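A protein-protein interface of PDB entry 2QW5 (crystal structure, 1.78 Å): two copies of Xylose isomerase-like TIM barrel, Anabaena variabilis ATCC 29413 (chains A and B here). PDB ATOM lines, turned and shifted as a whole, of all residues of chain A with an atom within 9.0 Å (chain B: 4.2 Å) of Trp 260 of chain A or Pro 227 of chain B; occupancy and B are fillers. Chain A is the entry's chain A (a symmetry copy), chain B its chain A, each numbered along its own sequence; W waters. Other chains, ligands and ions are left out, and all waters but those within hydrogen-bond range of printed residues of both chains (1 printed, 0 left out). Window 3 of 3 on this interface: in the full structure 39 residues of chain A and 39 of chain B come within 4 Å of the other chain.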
ATOM      1  N   SER A 217      27.867 -12.357   8.605  1.00  0.00           N
ATOM      2  CA  SER A 217      27.483 -11.154   7.854  1.00  0.00           C
ATOM      3  C   SER A 217      26.592 -10.177   8.636  1.00  0.00           C
ATOM      4  O   SER A 217      26.760  -8.962   8.488  1.00  0.00           O
ATOM      5  CB  SER A 217      26.804 -11.535   6.539  1.00  0.00           C
ATOM      6  OG  SER A 217      25.594 -12.282   6.768  1.00  0.00           O
ATOM      7  N   ALA A 218      25.670 -10.696   9.471  1.00  0.00           N
ATOM      8  CA  ALA A 218      24.802  -9.835  10.325  1.00  0.00           C
ATOM      9  C   ALA A 218      25.646  -8.982  11.279  1.00  0.00           C
ATOM     10  O   ALA A 218      25.447  -7.759  11.355  1.00  0.00           O
ATOM     11  CB  ALA A 218      23.809 -10.667  11.131  1.00  0.00           C
ATOM     12  N   ILE A 221      27.927  -6.349   9.220  1.00  0.00           N
ATOM     13  CA  ILE A 221      27.149  -5.204   8.767  1.00  0.00           C
ATOM     14  C   ILE A 221      26.774  -4.278   9.923  1.00  0.00           C
ATOM     15  O   ILE A 221      26.903  -3.056   9.768  1.00  0.00           O
ATOM     16  CB  ILE A 221      25.889  -5.652   8.033  1.00  0.00           C
ATOM     17  CG1 ILE A 221      26.209  -6.223   6.644  1.00  0.00           C
ATOM     18  CG2 ILE A 221      24.948  -4.405   7.772  1.00  0.00           C
ATOM     19  CD1 ILE A 221      27.670  -6.816   6.323  1.00  0.00           C
ATOM     20  N   LEU A 222      26.298  -4.842  11.052  1.00  0.00           N
ATOM     21  CA  LEU A 222      25.860  -4.021  12.196  1.00  0.00           C
ATOM     22  C   LEU A 222      26.971  -3.211  12.827  1.00  0.00           C
ATOM     23  O   LEU A 222      26.707  -2.092  13.269  1.00  0.00           O
ATOM     24  CB  LEU A 222      25.121  -4.820  13.288  1.00  0.00           C
ATOM     25  CG  LEU A 222      23.581  -4.830  13.147  1.00  0.00           C
ATOM     26  CD1 LEU A 222      23.154  -5.333  11.764  1.00  0.00           C
ATOM     27  CD2 LEU A 222      22.863  -5.588  14.307  1.00  0.00           C
ATOM     28  N   SER A 249      23.724 -14.405   7.343  1.00  0.00           N
ATOM     29  CA  SER A 249      22.594 -14.083   8.210  1.00  0.00           C
ATOM     30  C   SER A 249      22.204 -12.652   7.935  1.00  0.00           C
ATOM     31  O   SER A 249      23.096 -11.780   7.888  1.00  0.00           O
ATOM     32  CB  SER A 249      23.024 -14.178   9.668  1.00  0.00           C
ATOM     33  OG  SER A 249      21.909 -14.117  10.521  1.00  0.00           O
ATOM     34  N   PRO A 250      20.892 -12.372   7.787  1.00  0.00           N
ATOM     35  CA  PRO A 250      20.485 -11.016   7.469  1.00  0.00           C
ATOM     36  C   PRO A 250      20.601 -10.117   8.715  1.00  0.00           C
ATOM     37  O   PRO A 250      20.730 -10.634   9.823  1.00  0.00           O
ATOM     38  CB  PRO A 250      19.034 -11.218   7.013  1.00  0.00           C
ATOM     39  CG  PRO A 250      18.550 -12.303   7.812  1.00  0.00           C
ATOM     40  CD  PRO A 250      19.719 -13.236   7.975  1.00  0.00           C
ATOM     41  N   PRO A 251      20.586  -8.786   8.553  1.00  0.00           N
ATOM     42  CA  PRO A 251      20.680  -7.899   9.750  1.00  0.00           C
ATOM     43  C   PRO A 251      19.654  -8.130  10.860  1.00  0.00           C
ATOM     44  O   PRO A 251      20.004  -8.033  12.037  1.00  0.00           O
ATOM     45  CB  PRO A 251      20.491  -6.506   9.148  1.00  0.00           C
ATOM     46  CG  PRO A 251      21.112  -6.649   7.770  1.00  0.00           C
ATOM     47  CD  PRO A 251      20.586  -7.995   7.308  1.00  0.00           C
ATOM     48  N   ASP A 252      18.414  -8.476  10.484  1.00  0.00           N
ATOM     49  CA  ASP A 252      17.376  -8.740  11.480  1.00  0.00           C
ATOM     50  C   ASP A 252      17.382 -10.181  12.009  1.00  0.00           C
ATOM     51  O   ASP A 252      16.559 -10.506  12.838  1.00  0.00           O
ATOM     52  CB  ASP A 252      15.988  -8.315  10.972  1.00  0.00           C
ATOM     53  CG  ASP A 252      15.263  -9.401  10.171  1.00  0.00           C
ATOM     54  OD1 ASP A 252      15.907 -10.311   9.632  1.00  0.00           O
ATOM     55  OD2 ASP A 252      14.013  -9.302  10.091  1.00  0.00           O
ATOM     56  N   ALA A 255      14.526 -13.668   7.776  1.00  0.00           N
ATOM     57  CA  ALA A 255      14.458 -14.120   6.382  1.00  0.00           C
ATOM     58  C   ALA A 255      15.695 -13.691   5.610  1.00  0.00           C
ATOM     59  O   ALA A 255      15.974 -12.518   5.509  1.00  0.00           O
ATOM     60  CB  ALA A 255      13.218 -13.600   5.701  1.00  0.00           C
ATOM     61  N   LEU A 256      16.412 -14.649   5.039  1.00  0.00           N
ATOM     62  CA  LEU A 256      17.672 -14.328   4.335  1.00  0.00           C
ATOM     63  C   LEU A 256      17.449 -13.777   2.912  1.00  0.00           C
ATOM     64  O   LEU A 256      18.257 -13.007   2.390  1.00  0.00           O
ATOM     65  CB  LEU A 256      18.582 -15.565   4.380  1.00  0.00           C
ATOM     66  CG  LEU A 256      20.031 -15.481   3.900  1.00  0.00           C
ATOM     67  CD1 LEU A 256      20.811 -14.385   4.652  1.00  0.00           C
ATOM     68  CD2 LEU A 256      20.669 -16.863   4.049  1.00  0.00           C
ATOM     69  N   HIS A 257      16.305 -14.098   2.311  1.00  0.00           N
ATOM     70  CA  HIS A 257      16.029 -13.701   0.933  1.00  0.00           C
ATOM     71  C   HIS A 257      15.417 -12.306   0.736  1.00  0.00           C
ATOM     72  O   HIS A 257      15.312 -11.854  -0.413  1.00  0.00           O
ATOM     73  CB  HIS A 257      15.168 -14.761   0.225  1.00  0.00           C
ATOM     74  CG  HIS A 257      13.804 -14.921   0.800  1.00  0.00           C
ATOM     75  ND1 HIS A 257      13.589 -15.332   2.097  1.00  0.00           N
ATOM     76  CD2 HIS A 257      12.579 -14.795   0.231  1.00  0.00           C
ATOM     77  CE1 HIS A 257      12.287 -15.426   2.312  1.00  0.00           C
ATOM     78  NE2 HIS A 257      11.651 -15.104   1.195  1.00  0.00           N
ATOM     79  N   THR A 258      14.992 -11.643   1.826  1.00  0.00           N
ATOM     80  CA  THR A 258      14.457 -10.282   1.759  1.00  0.00           C
ATOM     81  C   THR A 258      15.227  -9.458   2.786  1.00  0.00           C
ATOM     82  O   THR A 258      14.831  -9.321   3.954  1.00  0.00           O
ATOM     83  CB  THR A 258      12.980 -10.288   2.034  1.00  0.00           C
ATOM     84  OG1 THR A 258      12.774 -10.882   3.315  1.00  0.00           O
ATOM     85  CG2 THR A 258      12.264 -11.103   0.983  1.00  0.00           C
ATOM     86  N   SER A 259      16.359  -8.936   2.365  1.00  0.00           N
ATOM     87  CA  SER A 259      17.191  -8.198   3.336  1.00  0.00           C
ATOM     88  C   SER A 259      18.225  -7.381   2.676  1.00  0.00           C
ATOM     89  O   SER A 259      18.443  -7.519   1.492  1.00  0.00           O
ATOM     90  CB  SER A 259      17.911  -9.170   4.293  1.00  0.00           C
ATOM     91  OG  SER A 259      19.051  -9.780   3.722  1.00  0.00           O
ATOM     92  N   TRP A 260      18.888  -6.562   3.504  1.00  0.00           N
ATOM     93  CA  TRP A 260      19.999  -5.724   3.071  1.00  0.00           C
ATOM     94  C   TRP A 260      21.401  -6.369   3.230  1.00  0.00           C
ATOM     95  O   TRP A 260      22.403  -5.655   3.257  1.00  0.00           O
ATOM     96  CB  TRP A 260      19.921  -4.394   3.805  1.00  0.00           C
ATOM     97  CG  TRP A 260      18.855  -3.521   3.269  1.00  0.00           C
ATOM     98  CD1 TRP A 260      17.577  -3.407   3.716  1.00  0.00           C
ATOM     99  CD2 TRP A 260      18.972  -2.651   2.139  1.00  0.00           C
ATOM    100  NE1 TRP A 260      16.896  -2.481   2.955  1.00  0.00           N
ATOM    101  CE2 TRP A 260      17.728  -2.008   1.977  1.00  0.00           C
ATOM    102  CE3 TRP A 260      20.039  -2.290   1.291  1.00  0.00           C
ATOM    103  CZ2 TRP A 260      17.497  -1.039   0.984  1.00  0.00           C
ATOM    104  CZ3 TRP A 260      19.797  -1.327   0.275  1.00  0.00           C
ATOM    105  CH2 TRP A 260      18.533  -0.722   0.146  1.00  0.00           C
ATOM    106  N   LEU A 261      21.489  -7.704   3.288  1.00  0.00           N
ATOM    107  CA  LEU A 261      22.795  -8.389   3.349  1.00  0.00           C
ATOM    108  C   LEU A 261      23.514  -8.046   2.043  1.00  0.00           C
ATOM    109  O   LEU A 261      22.981  -8.321   0.995  1.00  0.00           O
ATOM    110  CB  LEU A 261      22.643  -9.913   3.485  1.00  0.00           C
ATOM    111  CG  LEU A 261      23.867 -10.750   3.898  1.00  0.00           C
ATOM    112  CD1 LEU A 261      23.407 -12.160   4.053  1.00  0.00           C
ATOM    113  CD2 LEU A 261      25.061 -10.710   2.932  1.00  0.00           C
ATOM    114  N   PRO A 262      24.694  -7.418   2.106  1.00  0.00           N
ATOM    115  CA  PRO A 262      25.479  -7.010   0.936  1.00  0.00           C
ATOM    116  C   PRO A 262      26.244  -8.196   0.331  1.00  0.00           C
ATOM    117  O   PRO A 262      27.451  -8.352   0.487  1.00  0.00           O
ATOM    118  CB  PRO A 262      26.399  -5.934   1.520  1.00  0.00           C
ATOM    119  CG  PRO A 262      26.656  -6.372   2.876  1.00  0.00           C
ATOM    120  CD  PRO A 262      25.402  -7.058   3.355  1.00  0.00           C
ATOM    121  N   TRP A 263      25.495  -9.047  -0.341  1.00  0.00           N
ATOM    122  CA  TRP A 263      26.033 -10.284  -0.844  1.00  0.00           C
ATOM    123  C   TRP A 263      27.342 -10.196  -1.584  1.00  0.00           C
ATOM    124  O   TRP A 263      28.281 -10.943  -1.240  1.00  0.00           O
ATOM    125  CB  TRP A 263      25.015 -10.987  -1.725  1.00  0.00           C
ATOM    126  CG  TRP A 263      23.791 -11.401  -1.020  1.00  0.00           C
ATOM    127  CD1 TRP A 263      22.593 -10.730  -0.986  1.00  0.00           C
ATOM    128  CD2 TRP A 263      23.598 -12.612  -0.273  1.00  0.00           C
ATOM    129  NE1 TRP A 263      21.680 -11.451  -0.257  1.00  0.00           N
ATOM    130  CE2 TRP A 263      22.269 -12.604   0.199  1.00  0.00           C
ATOM    131  CE3 TRP A 263      24.431 -13.701   0.054  1.00  0.00           C
ATOM    132  CZ2 TRP A 263      21.746 -13.649   0.988  1.00  0.00           C
ATOM    133  CZ3 TRP A 263      23.918 -14.728   0.833  1.00  0.00           C
ATOM    134  CH2 TRP A 263      22.579 -14.707   1.271  1.00  0.00           C
ATOM    135  N   LYS A 264      27.414  -9.278  -2.548  1.00  0.00           N
ATOM    136  CA  LYS A 264      28.597  -9.160  -3.421  1.00  0.00           C
ATOM    137  C   LYS A 264      29.802  -8.692  -2.639  1.00  0.00           C
ATOM    138  O   LYS A 264      30.876  -9.323  -2.702  1.00  0.00           O
ATOM    139  CB  LYS A 264      28.336  -8.202  -4.587  1.00  0.00           C
ATOM    140  CG  LYS A 264      29.401  -8.165  -5.653  1.00  0.00           C
ATOM    141  CD  LYS A 264      29.106  -7.093  -6.698  1.00  0.00           C
ATOM    142  CE  LYS A 264      30.135  -7.177  -7.838  1.00  0.00           C
ATOM    143  NZ  LYS A 264      29.857  -6.252  -8.991  1.00  0.00           N
ATOM    144  N   SER A 265      29.613  -7.597  -1.898  1.00  0.00           N
ATOM    145  CA  SER A 265      30.700  -6.995  -1.098  1.00  0.00           C
ATOM    146  C   SER A 265      31.189  -7.809   0.062  1.00  0.00           C
ATOM    147  O   SER A 265      32.368  -7.712   0.441  1.00  0.00           O
ATOM    148  CB  SER A 265      30.277  -5.620  -0.611  1.00  0.00           C
ATOM    149  OG  SER A 265      30.397  -4.744  -1.689  1.00  0.00           O
ATOM    150  N   PHE A 266      30.295  -8.615   0.624  1.00  0.00           N
ATOM    151  CA  PHE A 266      30.620  -9.502   1.739  1.00  0.00           C
ATOM    152  C   PHE A 266      31.266 -10.797   1.228  1.00  0.00           C
ATOM    153  O   PHE A 266      32.305 -11.192   1.718  1.00  0.00           O
ATOM    154  CB  PHE A 266      29.368  -9.827   2.578  1.00  0.00           C
ATOM    155  CG  PHE A 266      29.646 -10.750   3.714  1.00  0.00           C
ATOM    156  CD1 PHE A 266      30.323 -10.280   4.849  1.00  0.00           C
ATOM    157  CD2 PHE A 266      29.288 -12.107   3.644  1.00  0.00           C
ATOM    158  CE1 PHE A 266      30.614 -11.141   5.913  1.00  0.00           C
ATOM    159  CE2 PHE A 266      29.586 -12.990   4.695  1.00  0.00           C
ATOM    160  CZ  PHE A 266      30.245 -12.492   5.849  1.00  0.00           C
ATOM    161  N   GLU A 328      23.397 -16.166  -5.173  1.00  0.00           N
ATOM    162  CA  GLU A 328      24.401 -15.123  -4.951  1.00  0.00           C
ATOM    163  C   GLU A 328      25.823 -15.617  -5.065  1.00  0.00           C
ATOM    164  O   GLU A 328      26.708 -14.874  -5.525  1.00  0.00           O
ATOM    165  CB  GLU A 328      24.136 -14.452  -3.602  1.00  0.00           C
ATOM    166  CG  GLU A 328      22.780 -13.705  -3.586  1.00  0.00           C
ATOM    167  CD  GLU A 328      22.713 -12.514  -4.529  1.00  0.00           C
ATOM    168  OE1 GLU A 328      23.762 -11.888  -4.830  1.00  0.00           O
ATOM    169  OE2 GLU A 328      21.579 -12.203  -4.949  1.00  0.00           O
ATOM    170  N   GLU B 220      16.592   1.292   7.908  1.00  0.00           N
ATOM    171  CA  GLU B 220      16.254   0.529   6.675  1.00  0.00           C
ATOM    172  C   GLU B 220      17.114  -0.732   6.546  1.00  0.00           C
ATOM    173  O   GLU B 220      16.606  -1.832   6.314  1.00  0.00           O
ATOM    174  CB  GLU B 220      16.387   1.394   5.422  1.00  0.00           C
ATOM    175  CG  GLU B 220      16.004   0.687   4.093  1.00  0.00           C
ATOM    176  CD  GLU B 220      14.610   0.120   4.117  1.00  0.00           C
ATOM    177  OE1 GLU B 220      13.736   0.772   4.718  1.00  0.00           O
ATOM    178  OE2 GLU B 220      14.389  -0.966   3.530  1.00  0.00           O
ATOM    179  N   ILE B 221      18.411  -0.585   6.792  1.00  0.00           N
ATOM    180  CA  ILE B 221      19.339  -1.705   6.717  1.00  0.00           C
ATOM    181  C   ILE B 221      19.076  -2.736   7.813  1.00  0.00           C
ATOM    182  O   ILE B 221      19.076  -3.936   7.508  1.00  0.00           O
ATOM    183  CB  ILE B 221      20.785  -1.226   6.794  1.00  0.00           C
ATOM    184  CG1 ILE B 221      21.226  -0.529   5.498  1.00  0.00           C
ATOM    185  CG2 ILE B 221      21.754  -2.468   6.957  1.00  0.00           C
ATOM    186  CD1 ILE B 221      20.135   0.126   4.512  1.00  0.00           C
ATOM    187  N   GLY B 224      14.822  -3.595   7.130  1.00  0.00           N
ATOM    188  CA  GLY B 224      14.163  -3.569   5.825  1.00  0.00           C
ATOM    189  C   GLY B 224      14.295  -4.816   4.984  1.00  0.00           C
ATOM    190  O   GLY B 224      15.063  -5.722   5.275  1.00  0.00           O
ATOM    191  N   GLU B 225      13.596  -4.787   3.869  1.00  0.00           N
ATOM    192  CA  GLU B 225      13.412  -5.953   3.019  1.00  0.00           C
ATOM    193  C   GLU B 225      14.318  -6.081   1.808  1.00  0.00           C
ATOM    194  O   GLU B 225      14.112  -6.981   0.959  1.00  0.00           O
ATOM    195  CB  GLU B 225      11.918  -5.989   2.646  1.00  0.00           C
ATOM    196  CG  GLU B 225      11.054  -6.164   3.885  1.00  0.00           C
ATOM    197  CD  GLU B 225       9.564  -6.154   3.628  1.00  0.00           C
ATOM    198  OE1 GLU B 225       9.017  -5.096   3.273  1.00  0.00           O
ATOM    199  OE2 GLU B 225       8.923  -7.203   3.873  1.00  0.00           O
ATOM    200  N   GLY B 226      15.361  -5.259   1.739  1.00  0.00           N
ATOM    201  CA  GLY B 226      16.288  -5.314   0.634  1.00  0.00           C
ATOM    202  C   GLY B 226      16.050  -4.282  -0.466  1.00  0.00           C
ATOM    203  O   GLY B 226      14.948  -3.651  -0.575  1.00  0.00           O
ATOM    204  N   PRO B 227      17.053  -4.123  -1.325  1.00  0.00           N
ATOM    205  CA  PRO B 227      16.969  -3.057  -2.328  1.00  0.00           C
ATOM    206  C   PRO B 227      15.817  -3.098  -3.350  1.00  0.00           C
ATOM    207  O   PRO B 227      15.337  -2.009  -3.737  1.00  0.00           O
ATOM    208  CB  PRO B 227      18.366  -3.056  -2.946  1.00  0.00           C
ATOM    209  CG  PRO B 227      18.888  -4.375  -2.703  1.00  0.00           C
ATOM    210  CD  PRO B 227      18.328  -4.852  -1.422  1.00  0.00           C
ATOM    211  N   GLU B 228      15.335  -4.295  -3.726  1.00  0.00           N
ATOM    212  CA  GLU B 228      14.253  -4.394  -4.733  1.00  0.00           C
ATOM    213  C   GLU B 228      12.926  -3.930  -4.165  1.00  0.00           C
ATOM    214  O   GLU B 228      12.257  -3.100  -4.776  1.00  0.00           O
ATOM    215  CB  GLU B 228      14.101  -5.803  -5.371  1.00  0.00           C
ATOM    216  CG  GLU B 228      15.284  -6.292  -6.177  1.00  0.00           C
ATOM    217  CD  GLU B 228      16.457  -6.808  -5.333  1.00  0.00           C
ATOM    218  OE1 GLU B 228      16.299  -7.130  -4.115  1.00  0.00           O
ATOM    219  OE2 GLU B 228      17.566  -6.893  -5.906  1.00  0.00           O
ATOM    220  N   ILE B 229      12.550  -4.473  -3.002  1.00  0.00           N
ATOM    221  CA  ILE B 229      11.330  -4.064  -2.301  1.00  0.00           C
ATOM    222  C   ILE B 229      11.445  -2.587  -1.875  1.00  0.00           C
ATOM    223  O   ILE B 229      10.519  -1.831  -2.056  1.00  0.00           O
ATOM    224  CB  ILE B 229      11.038  -4.986  -1.118  1.00  0.00           C
ATOM    225  CG1 ILE B 229      10.640  -6.372  -1.659  1.00  0.00           C
ATOM    226  CG2 ILE B 229       9.951  -4.394  -0.207  1.00  0.00           C
ATOM    227  CD1 ILE B 229      10.750  -7.511  -0.637  1.00  0.00           C
ATOM    228  N   PHE B 230      12.613  -2.167  -1.389  1.00  0.00           N
ATOM    229  CA  PHE B 230      12.836  -0.768  -1.009  1.00  0.00           C
ATOM    230  C   PHE B 230      12.596   0.269  -2.124  1.00  0.00           C
ATOM    231  O   PHE B 230      11.968   1.314  -1.873  1.00  0.00           O
ATOM    232  CB  PHE B 230      14.246  -0.613  -0.476  1.00  0.00           C
ATOM    233  CG  PHE B 230      14.596   0.793  -0.111  1.00  0.00           C
ATOM    234  CD1 PHE B 230      13.960   1.413   0.968  1.00  0.00           C
ATOM    235  CD2 PHE B 230      15.589   1.493  -0.807  1.00  0.00           C
ATOM    236  CE1 PHE B 230      14.305   2.710   1.339  1.00  0.00           C
ATOM    237  CE2 PHE B 230      15.922   2.777  -0.447  1.00  0.00           C
ATOM    238  CZ  PHE B 230      15.276   3.389   0.618  1.00  0.00           C
ATOM    239  N   LYS B 231      13.072  -0.047  -3.326  1.00  0.00           N
ATOM    240  CA  LYS B 231      12.870   0.773  -4.512  1.00  0.00           C
ATOM    241  C   LYS B 231      11.365   0.970  -4.801  1.00  0.00           C
ATOM    242  O   LYS B 231      10.943   2.078  -5.110  1.00  0.00           O
ATOM    243  CB  LYS B 231      13.636   0.170  -5.716  1.00  0.00           C
ATOM    244  CG  LYS B 231      13.556   1.014  -7.005  1.00  0.00           C
ATOM    245  CD  LYS B 231      14.342   0.483  -8.220  1.00  0.00           C
ATOM    246  CE  LYS B 231      13.923   1.268  -9.499  1.00  0.00           C
ATOM    247  NZ  LYS B 231      14.702   0.961 -10.725  1.00  0.00           N
ATOM    248  N   PRO B 262      24.863   1.017   2.549  1.00  0.00           N
ATOM    249  CA  PRO B 262      24.817   0.732   1.112  1.00  0.00           C
ATOM    250  C   PRO B 262      24.454   1.984   0.301  1.00  0.00           C
ATOM    251  O   PRO B 262      23.341   2.155  -0.186  1.00  0.00           O
ATOM    252  CB  PRO B 262      23.755  -0.368   1.032  1.00  0.00           C
ATOM    253  CG  PRO B 262      22.815  -0.043   2.084  1.00  0.00           C
ATOM    254  CD  PRO B 262      23.615   0.568   3.206  1.00  0.00           C
ATOM    255  N   SER B 265      22.768   1.663  -3.405  1.00  0.00           N
ATOM    256  CA  SER B 265      21.437   1.021  -3.348  1.00  0.00           C
ATOM    257  C   SER B 265      20.393   1.744  -2.550  1.00  0.00           C
ATOM    258  O   SER B 265      19.194   1.642  -2.855  1.00  0.00           O
ATOM    259  CB  SER B 265      21.576  -0.401  -2.833  1.00  0.00           C
ATOM    260  OG  SER B 265      22.060  -1.177  -3.885  1.00  0.00           O
HETATM  261  O   HOH W   1      17.749  -5.890   6.213  1.00  0.00           O
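Water W1 lies within hydrogen-bond range of the backbone carbonyl oxygen (O) of Ile 221 of chain B, the backbone carbonyl oxygen (O) of Gly 224 of chain B and the backbone NH (N) of Trp 260 of chain A.
Pro 251 of chain A touches Ile 221 of chain B.
Thr 258 of chain A touches Glu 225 of chain B.
O of Gly 224 of chain B touches CA of Ser 259 of chain A, at 3.8 Å.
O of Ser 259 of chain A touches CA of Gly 226 of chain B, 3.2 Å away.
Pro 227 of chain B touches Ser 259 of chain A (CD to O, 3.95 Å).
CD1 of Trp 260 of chain A touches O of Gly 224 of chain B, 3.8 Å away.
Trp 260 of chain A touches Pro 227 of chain B (CH2 to CA, 3.7 Å).
Phe 230 of chain B touches Trp 260 of chain A.
Trp 260 of chain A touches Pro 262 of chain B.
Trp 260 of chain A touches Ser 265 of chain B.
The backbone NH (N) of Leu 261 of chain A sits at hydrogen-bond distance from the side-chain hydroxyl (OG) of Ser 259 of chain A.
Of the 12 printed residues of chain B, 9 touch a printed residue of chain A.
Printed residues of chain B that touch a printed residue of chain A: Glu 220, Ile 221, Gly 224, Glu 225, Gly 226, Pro 227, Phe 230, Pro 262 and Ser 265.
Hydrophobic or aromatic side chains of chain B within 4 Å of the printed part of chain A: Ile 221, Pro 227, Phe 230 and Pro 262.
Of the 21 printed residues of chain A, 5 touch a printed residue of chain B.
Printed residues of chain A that touch a printed residue of chain B: Ile 221, Pro 251, Thr 258, Ser 259 and Trp 260.
Hydrophobic or aromatic side chains of chain A that line the printed part of chain B: Ile 221, Pro 251 and Trp 260.
Along chain A the printed residues that touch a printed residue of chain B span positions 221 to 260.
Among the printed residues, no Asp or Glu carboxylate lies within 4 Å of a Lys or Arg side-chain nitrogen of the other chain.
Ala 218 of chain A touches none of the printed residues of chain B.
Of the printed residues of chain B, Pro 251 of chain A touches Ile 221.
Printed residues of chain B within 4 Å of Thr 258 of chain A: Gly 224 and Glu 225.
Of the printed residues of chain B, Trp 260 of chain A touches Glu 220 (3.0 Å), Ile 221 (3.8 Å), Gly 224 (3.8 Å), Gly 226 (3.4 Å), Pro 227 (3.7 Å), Phe 230 (3.6 Å), Pro 262 (3.7 Å) and Ser 265 (3.7 Å).
Of the printed residues of chain A, Glu 220 of chain B touches Trp 260.
Ile 221 of chain B touches just these residues of chain A: Ile 221, Pro 251 and Trp 260.
Gly 226 of chain B touches two residues of chain A.
Pro 227 of chain B touches just these residues of chain A: Ser 259 (3.95 Å) and Trp 260 (3.7 Å).
Of the printed residues of chain A, Phe 230 of chain B touches Trp 260.
Lys 231 of chain B touches none of the printed residues of chain A.
Of the printed residues of chain A, Ser 265 of chain B touches Trp 260 (3.7 Å).
The side-chain carboxylate of Glu 220 of chain B sits at hydrogen-bond distance from the indole nitrogen of Trp 260 of chain A, at 3.0 Å.
The backbone carbonyl oxygen (O) of Glu 225 of chain B sits at hydrogen-bond distance from the backbone NH (N) of Ser 259 of chain A.
The indole nitrogen (NE1) of Trp 260 of chain A lies close to the backbone NH (N) of Gly 226 of chain B, 3.4 Å away.
Ile 221 of chain B touches its own counterpart, Ile 221 of chain A.
Positions printed for both chains: 221, 262 and 265.
Of the 16 pairs that touch across the chains among the printed residues, 1 has its exchanged pair printed and touching as well.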
